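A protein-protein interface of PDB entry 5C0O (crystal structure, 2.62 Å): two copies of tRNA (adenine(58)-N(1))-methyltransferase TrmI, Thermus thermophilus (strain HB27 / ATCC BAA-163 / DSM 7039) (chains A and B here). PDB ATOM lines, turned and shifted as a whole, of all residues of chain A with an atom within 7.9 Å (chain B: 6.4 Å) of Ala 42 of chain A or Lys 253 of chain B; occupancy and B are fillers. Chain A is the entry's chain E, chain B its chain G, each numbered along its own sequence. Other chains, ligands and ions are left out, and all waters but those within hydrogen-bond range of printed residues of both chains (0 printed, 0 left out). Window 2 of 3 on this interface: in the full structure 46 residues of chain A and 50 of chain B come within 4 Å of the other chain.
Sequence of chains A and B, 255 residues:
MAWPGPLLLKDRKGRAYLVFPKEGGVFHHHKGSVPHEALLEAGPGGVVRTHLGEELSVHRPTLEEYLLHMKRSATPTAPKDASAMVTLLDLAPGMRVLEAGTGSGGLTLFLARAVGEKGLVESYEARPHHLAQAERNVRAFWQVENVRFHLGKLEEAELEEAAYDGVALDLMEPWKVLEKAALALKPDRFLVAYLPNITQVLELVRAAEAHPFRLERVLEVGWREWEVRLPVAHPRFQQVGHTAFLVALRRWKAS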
ATOM      1  N   LEU A   7      25.956  23.812  26.937  1.00  0.00           N
ATOM      2  CA  LEU A   7      25.086  22.644  26.887  1.00  0.00           C
ATOM      3  C   LEU A   7      23.662  23.034  27.258  1.00  0.00           C
ATOM      4  O   LEU A   7      23.450  24.018  27.968  1.00  0.00           O
ATOM      5  CB  LEU A   7      25.585  21.564  27.845  1.00  0.00           C
ATOM      6  CG  LEU A   7      26.228  20.298  27.279  1.00  0.00           C
ATOM      7  CD1 LEU A   7      27.534  20.579  26.555  1.00  0.00           C
ATOM      8  CD2 LEU A   7      26.463  19.330  28.416  1.00  0.00           C
ATOM      9  N   HIS A  36      28.811  17.939  36.268  1.00  0.00           N
ATOM     10  CA  HIS A  36      29.028  18.451  34.916  1.00  0.00           C
ATOM     11  C   HIS A  36      29.709  17.459  33.979  1.00  0.00           C
ATOM     12  O   HIS A  36      29.166  17.144  32.921  1.00  0.00           O
ATOM     13  CB  HIS A  36      29.846  19.741  34.969  1.00  0.00           C
ATOM     14  CG  HIS A  36      29.008  20.975  35.096  1.00  0.00           C
ATOM     15  ND1 HIS A  36      29.480  22.232  34.784  1.00  0.00           N
ATOM     16  CD2 HIS A  36      27.727  21.143  35.498  1.00  0.00           C
ATOM     17  CE1 HIS A  36      28.526  23.121  34.993  1.00  0.00           C
ATOM     18  NE2 HIS A  36      27.451  22.487  35.425  1.00  0.00           N
ATOM     19  N   GLU A  37      30.891  16.970  34.346  1.00  0.00           N
ATOM     20  CA  GLU A  37      31.604  16.037  33.475  1.00  0.00           C
ATOM     21  C   GLU A  37      30.823  14.737  33.294  1.00  0.00           C
ATOM     22  O   GLU A  37      31.156  13.920  32.435  1.00  0.00           O
ATOM     23  CB  GLU A  37      33.008  15.737  34.009  1.00  0.00           C
ATOM     24  CG  GLU A  37      33.081  15.409  35.487  1.00  0.00           C
ATOM     25  CD  GLU A  37      33.745  16.513  36.287  1.00  0.00           C
ATOM     26  OE1 GLU A  37      34.990  16.608  36.246  1.00  0.00           O
ATOM     27  OE2 GLU A  37      33.021  17.287  36.947  1.00  0.00           O
ATOM     28  N   ALA A  38      29.787  14.551  34.106  1.00  0.00           N
ATOM     29  CA  ALA A  38      28.860  13.440  33.933  1.00  0.00           C
ATOM     30  C   ALA A  38      27.950  13.687  32.730  1.00  0.00           C
ATOM     31  O   ALA A  38      27.503  12.744  32.074  1.00  0.00           O
ATOM     32  CB  ALA A  38      28.039  13.238  35.191  1.00  0.00           C
ATOM     33  N   LEU A  39      27.677  14.959  32.449  1.00  0.00           N
ATOM     34  CA  LEU A  39      26.915  15.339  31.265  1.00  0.00           C
ATOM     35  C   LEU A  39      27.762  15.160  30.014  1.00  0.00           C
ATOM     36  O   LEU A  39      27.290  14.649  28.998  1.00  0.00           O
ATOM     37  CB  LEU A  39      26.443  16.791  31.357  1.00  0.00           C
ATOM     38  CG  LEU A  39      25.551  17.171  32.534  1.00  0.00           C
ATOM     39  CD1 LEU A  39      25.382  18.678  32.565  1.00  0.00           C
ATOM     40  CD2 LEU A  39      24.206  16.464  32.437  1.00  0.00           C
ATOM     41  N   LEU A  40      29.015  15.595  30.099  1.00  0.00           N
ATOM     42  CA  LEU A  40      29.944  15.510  28.982  1.00  0.00           C
ATOM     43  C   LEU A  40      30.097  14.068  28.518  1.00  0.00           C
ATOM     44  O   LEU A  40      30.055  13.782  27.322  1.00  0.00           O
ATOM     45  CB  LEU A  40      31.312  16.072  29.371  1.00  0.00           C
ATOM     46  CG  LEU A  40      31.372  17.458  30.016  1.00  0.00           C
ATOM     47  CD1 LEU A  40      32.797  17.752  30.462  1.00  0.00           C
ATOM     48  CD2 LEU A  40      30.883  18.532  29.062  1.00  0.00           C
ATOM     49  N   GLU A  41      30.265  13.163  29.476  1.00  0.00           N
ATOM     50  CA  GLU A  41      30.510  11.762  29.166  1.00  0.00           C
ATOM     51  C   GLU A  41      29.289  11.144  28.493  1.00  0.00           C
ATOM     52  O   GLU A  41      29.417  10.234  27.673  1.00  0.00           O
ATOM     53  CB  GLU A  41      30.883  10.990  30.432  1.00  0.00           C
ATOM     54  CG  GLU A  41      32.232  10.289  30.346  1.00  0.00           C
ATOM     55  CD  GLU A  41      32.887  10.117  31.702  1.00  0.00           C
ATOM     56  OE1 GLU A  41      33.697  10.989  32.084  1.00  0.00           O
ATOM     57  OE2 GLU A  41      32.593   9.116  32.388  1.00  0.00           O
ATOM     58  N   ALA A  42      28.108  11.643  28.839  1.00  0.00           N
ATOM     59  CA  ALA A  42      26.899  11.280  28.113  1.00  0.00           C
ATOM     60  C   ALA A  42      26.883  12.046  26.794  1.00  0.00           C
ATOM     61  O   ALA A  42      26.875  11.452  25.722  1.00  0.00           O
ATOM     62  CB  ALA A  42      25.657  11.581  28.937  1.00  0.00           C
ATOM     63  N   GLY A  43      26.892  13.372  26.879  1.00  0.00           N
ATOM     64  CA  GLY A  43      27.055  14.212  25.705  1.00  0.00           C
ATOM     65  C   GLY A  43      25.781  14.426  24.908  1.00  0.00           C
ATOM     66  O   GLY A  43      24.794  13.724  25.119  1.00  0.00           O
ATOM     67  N   PRO A  44      25.806  15.396  23.976  1.00  0.00           N
ATOM     68  CA  PRO A  44      24.662  15.778  23.135  1.00  0.00           C
ATOM     69  C   PRO A  44      23.893  14.584  22.584  1.00  0.00           C
ATOM     70  O   PRO A  44      24.480  13.706  21.948  1.00  0.00           O
ATOM     71  CB  PRO A  44      25.316  16.574  22.003  1.00  0.00           C
ATOM     72  CG  PRO A  44      26.525  17.170  22.626  1.00  0.00           C
ATOM     73  CD  PRO A  44      27.017  16.159  23.624  1.00  0.00           C
ATOM     74  N   GLY A  45      22.588  14.558  22.837  1.00  0.00           N
ATOM     75  CA  GLY A  45      21.750  13.436  22.458  1.00  0.00           C
ATOM     76  C   GLY A  45      21.715  12.393  23.558  1.00  0.00           C
ATOM     77  O   GLY A  45      20.824  11.543  23.595  1.00  0.00           O
ATOM     78  N   GLY A  46      22.690  12.464  24.459  1.00  0.00           N
ATOM     79  CA  GLY A  46      22.778  11.536  25.568  1.00  0.00           C
ATOM     80  C   GLY A  46      21.701  11.791  26.599  1.00  0.00           C
ATOM     81  O   GLY A  46      20.826  12.637  26.402  1.00  0.00           O
ATOM     82  N   VAL A  47      21.769  11.054  27.703  1.00  0.00           N
ATOM     83  CA  VAL A  47      20.791  11.177  28.774  1.00  0.00           C
ATOM     84  C   VAL A  47      21.453  10.840  30.111  1.00  0.00           C
ATOM     85  O   VAL A  47      22.308   9.955  30.179  1.00  0.00           O
ATOM     86  CB  VAL A  47      19.564  10.260  28.519  1.00  0.00           C
ATOM     87  CG1 VAL A  47      19.962   8.780  28.513  1.00  0.00           C
ATOM     88  CG2 VAL A  47      18.469  10.524  29.541  1.00  0.00           C
ATOM     89  N   VAL A  48      21.081  11.569  31.161  1.00  0.00           N
ATOM     90  CA  VAL A  48      21.624  11.334  32.497  1.00  0.00           C
ATOM     91  C   VAL A  48      20.501  11.207  33.524  1.00  0.00           C
ATOM     92  O   VAL A  48      19.444  11.821  33.383  1.00  0.00           O
ATOM     93  CB  VAL A  48      22.590  12.467  32.929  1.00  0.00           C
ATOM     94  CG1 VAL A  48      21.837  13.781  33.137  1.00  0.00           C
ATOM     95  CG2 VAL A  48      23.347  12.072  34.191  1.00  0.00           C
ATOM     96  N   LEU A  56      17.056  13.203  32.398  1.00  0.00           N
ATOM     97  CA  LEU A  56      17.459  14.497  31.858  1.00  0.00           C
ATOM     98  C   LEU A  56      18.287  14.305  30.589  1.00  0.00           C
ATOM     99  O   LEU A  56      19.235  13.522  30.579  1.00  0.00           O
ATOM    100  CB  LEU A  56      18.260  15.282  32.899  1.00  0.00           C
ATOM    101  CG  LEU A  56      17.489  15.838  34.100  1.00  0.00           C
ATOM    102  CD1 LEU A  56      17.090  14.749  35.095  1.00  0.00           C
ATOM    103  CD2 LEU A  56      18.315  16.912  34.788  1.00  0.00           C
ATOM    104  N   SER A  57      17.927  15.024  29.528  1.00  0.00           N
ATOM    105  CA  SER A  57      18.598  14.876  28.237  1.00  0.00           C
ATOM    106  C   SER A  57      19.470  16.089  27.920  1.00  0.00           C
ATOM    107  O   SER A  57      19.085  17.229  28.167  1.00  0.00           O
ATOM    108  CB  SER A  57      17.570  14.656  27.123  1.00  0.00           C
ATOM    109  OG  SER A  57      16.666  15.743  27.028  1.00  0.00           O
ATOM    110  N   VAL A  58      20.636  15.815  27.343  1.00  0.00           N
ATOM    111  CA  VAL A  58      21.692  16.809  27.163  1.00  0.00           C
ATOM    112  C   VAL A  58      21.909  17.105  25.671  1.00  0.00           C
ATOM    113  O   VAL A  58      21.850  16.204  24.832  1.00  0.00           O
ATOM    114  CB  VAL A  58      23.024  16.334  27.850  1.00  0.00           C
ATOM    115  CG1 VAL A  58      23.289  14.828  27.646  1.00  0.00           C
ATOM    116  CG2 VAL A  58      24.224  17.136  27.370  1.00  0.00           C
ATOM    117  N   PRO B 187      24.518  12.606  16.736  1.00  0.00           N
ATOM    118  CA  PRO B 187      23.650  12.818  17.895  1.00  0.00           C
ATOM    119  C   PRO B 187      23.240  14.277  18.043  1.00  0.00           C
ATOM    120  O   PRO B 187      24.066  15.166  17.831  1.00  0.00           O
ATOM    121  CB  PRO B 187      24.525  12.373  19.070  1.00  0.00           C
ATOM    122  CG  PRO B 187      25.422  11.344  18.484  1.00  0.00           C
ATOM    123  CD  PRO B 187      25.705  11.804  17.079  1.00  0.00           C
ATOM    124  N   ASP B 188      21.972  14.507  18.374  1.00  0.00           N
ATOM    125  CA  ASP B 188      21.473  15.839  18.708  1.00  0.00           C
ATOM    126  C   ASP B 188      21.239  16.728  17.482  1.00  0.00           C
ATOM    127  O   ASP B 188      20.896  17.901  17.631  1.00  0.00           O
ATOM    128  CB  ASP B 188      22.447  16.538  19.663  1.00  0.00           C
ATOM    129  CG  ASP B 188      21.742  17.354  20.727  1.00  0.00           C
ATOM    130  OD1 ASP B 188      20.789  16.839  21.353  1.00  0.00           O
ATOM    131  OD2 ASP B 188      22.149  18.515  20.936  1.00  0.00           O
ATOM    132  N   ARG B 214      13.405  11.716  18.586  1.00  0.00           N
ATOM    133  CA  ARG B 214      12.602  12.397  19.594  1.00  0.00           C
ATOM    134  C   ARG B 214      11.975  13.634  18.960  1.00  0.00           C
ATOM    135  O   ARG B 214      12.656  14.642  18.764  1.00  0.00           O
ATOM    136  CB  ARG B 214      13.470  12.791  20.801  1.00  0.00           C
ATOM    137  CG  ARG B 214      14.933  13.026  20.421  1.00  0.00           C
ATOM    138  CD  ARG B 214      15.788  13.730  21.472  1.00  0.00           C
ATOM    139  NE  ARG B 214      15.635  13.209  22.831  1.00  0.00           N
ATOM    140  CZ  ARG B 214      16.373  12.240  23.373  1.00  0.00           C
ATOM    141  NH1 ARG B 214      17.328  11.631  22.677  1.00  0.00           N
ATOM    142  NH2 ARG B 214      16.143  11.869  24.625  1.00  0.00           N
ATOM    143  N   ARG B 251      17.813  13.539  16.656  1.00  0.00           N
ATOM    144  CA  ARG B 251      18.276  12.159  16.750  1.00  0.00           C
ATOM    145  C   ARG B 251      18.802  11.803  18.140  1.00  0.00           C
ATOM    146  O   ARG B 251      19.313  12.661  18.862  1.00  0.00           O
ATOM    147  CB  ARG B 251      19.367  11.900  15.707  1.00  0.00           C
ATOM    148  CG  ARG B 251      19.943  10.500  15.779  1.00  0.00           C
ATOM    149  CD  ARG B 251      20.684  10.103  14.519  1.00  0.00           C
ATOM    150  NE  ARG B 251      20.706   8.650  14.372  1.00  0.00           N
ATOM    151  CZ  ARG B 251      21.575   7.842  14.972  1.00  0.00           C
ATOM    152  NH1 ARG B 251      22.524   8.334  15.759  1.00  0.00           N
ATOM    153  NH2 ARG B 251      21.501   6.533  14.772  1.00  0.00           N
ATOM    154  N   TRP B 252      18.671  10.529  18.502  1.00  0.00           N
ATOM    155  CA  TRP B 252      19.210  10.009  19.756  1.00  0.00           C
ATOM    156  C   TRP B 252      20.707   9.792  19.648  1.00  0.00           C
ATOM    157  O   TRP B 252      21.211   9.437  18.585  1.00  0.00           O
ATOM    158  CB  TRP B 252      18.553   8.677  20.136  1.00  0.00           C
ATOM    159  CG  TRP B 252      17.075   8.733  20.240  1.00  0.00           C
ATOM    160  CD1 TRP B 252      16.314   9.848  20.338  1.00  0.00           C
ATOM    161  CD2 TRP B 252      16.170   7.623  20.250  1.00  0.00           C
ATOM    162  NE1 TRP B 252      14.984   9.514  20.411  1.00  0.00           N
ATOM    163  CE2 TRP B 252      14.870   8.150  20.358  1.00  0.00           C
ATOM    164  CE3 TRP B 252      16.335   6.235  20.183  1.00  0.00           C
ATOM    165  CZ2 TRP B 252      13.736   7.341  20.397  1.00  0.00           C
ATOM    166  CZ3 TRP B 252      15.205   5.431  20.218  1.00  0.00           C
ATOM    167  CH2 TRP B 252      13.924   5.987  20.326  1.00  0.00           C
ATOM    168  N   LYS B 253      21.421   9.984  20.749  1.00  0.00           N
ATOM    169  CA  LYS B 253      22.793   9.515  20.807  1.00  0.00           C
ATOM    170  C   LYS B 253      22.720   8.000  20.919  1.00  0.00           C
ATOM    171  O   LYS B 253      22.266   7.472  21.933  1.00  0.00           O
ATOM    172  CB  LYS B 253      23.558  10.129  21.978  1.00  0.00           C
ATOM    173  CG  LYS B 253      25.048   9.842  21.928  1.00  0.00           C
ATOM    174  CD  LYS B 253      25.438   8.719  22.868  1.00  0.00           C
ATOM    175  CE  LYS B 253      25.856   9.284  24.207  1.00  0.00           C
ATOM    176  NZ  LYS B 253      25.770   8.313  25.329  1.00  0.00           N
ATOM    177  N   ALA B 254      23.140   7.313  19.859  1.00  0.00           N
ATOM    178  CA  ALA B 254      22.980   5.866  19.742  1.00  0.00           C
ATOM    179  C   ALA B 254      23.402   5.097  20.990  1.00  0.00           C
ATOM    180  O   ALA B 254      22.558   4.646  21.766  1.00  0.00           O
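N of Lys 253 of chain B is in hydrogen-bond range of O of Gly 45 of chain A, 3.3 Å away.
N of Gly 45 of chain A is in hydrogen-bond range of OD1 of Asp 188 of chain B, at 3.3 Å.
The backbone carbonyl oxygen (O) of Ala 42 of chain A sits close to the side-chain amino group (NZ) of Lys 253 of chain B, 3.4 Å away.
N of Asp 188 of chain B sits at hydrogen-bond distance from O of Arg 251 of chain B, 3.3 Å away.
O of Gly 46 of chain A is in hydrogen-bond range of N of Val 58 of chain A (3.3 Å).
The backbone carbonyl oxygen (O) of Val 58 of chain A sits at hydrogen-bond distance from the backbone NH (N) of Gly 45 of chain A (2.7 Å).
Among the printed residues, pairs that only touch across the chains: Pro 44 of chain A with Pro 187 of chain B (3.2 Å), Pro 44 of chain A with Asp 188 of chain B (3.7 Å), Pro 44 of chain A with Lys 253 of chain B (3.7 Å), Gly 45 of chain A with Arg 214 of chain B (3.6 Å), Gly 46 of chain A with Lys 253 of chain B (3.5 Å) and Val 58 of chain A with Asp 188 of chain B (3.7 Å).
Ala 42 of chain A touches one residue of chain B.
Lys 253 of chain B touches just these residues of chain A: Ala 42 (2.8 Å), Pro 44 (3.7 Å), Gly 45 (3.3 Å) and Gly 46 (3.5 Å).
Printed residues of chain A within 4 Å of Arg 214 of chain B: Gly 45 (3.6 Å).
Of the printed residues of chain B, Gly 45 of chain A touches Asp 188, Arg 214 and Lys 253.
Printed residues of chain A within 4 Å of Asp 188 of chain B: Pro 44 (3.7 Å), Gly 45 (3.3 Å) and Val 58 (3.7 Å).
Printed residues of chain B within 4 Å of Gly 46 of chain A: Lys 253 (3.5 Å).
Of the printed residues of chain B, Pro 44 of chain A touches Pro 187 (3.2 Å), Asp 188 (3.7 Å) and Lys 253 (3.7 Å).
Of the 7 printed residues of chain B, 4 touch a printed residue of chain A.
Hydrophobic or aromatic side chains of chain B within 4 Å of the printed part of chain A: Pro 187.
Hydrophobic or aromatic side chains of chain A that line the printed part of chain B: Pro 44.
Among the printed residues, 9 pairs touch across the chains.
Among the printed residues, no Asp or Glu carboxylate lies within 4 Å of a Lys or Arg side-chain nitrogen of the other chain.
No position is printed for both chains.
Of the 9 pairs that touch across the chains among the printed residues, none has its exchanged pair printed and touching as well.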
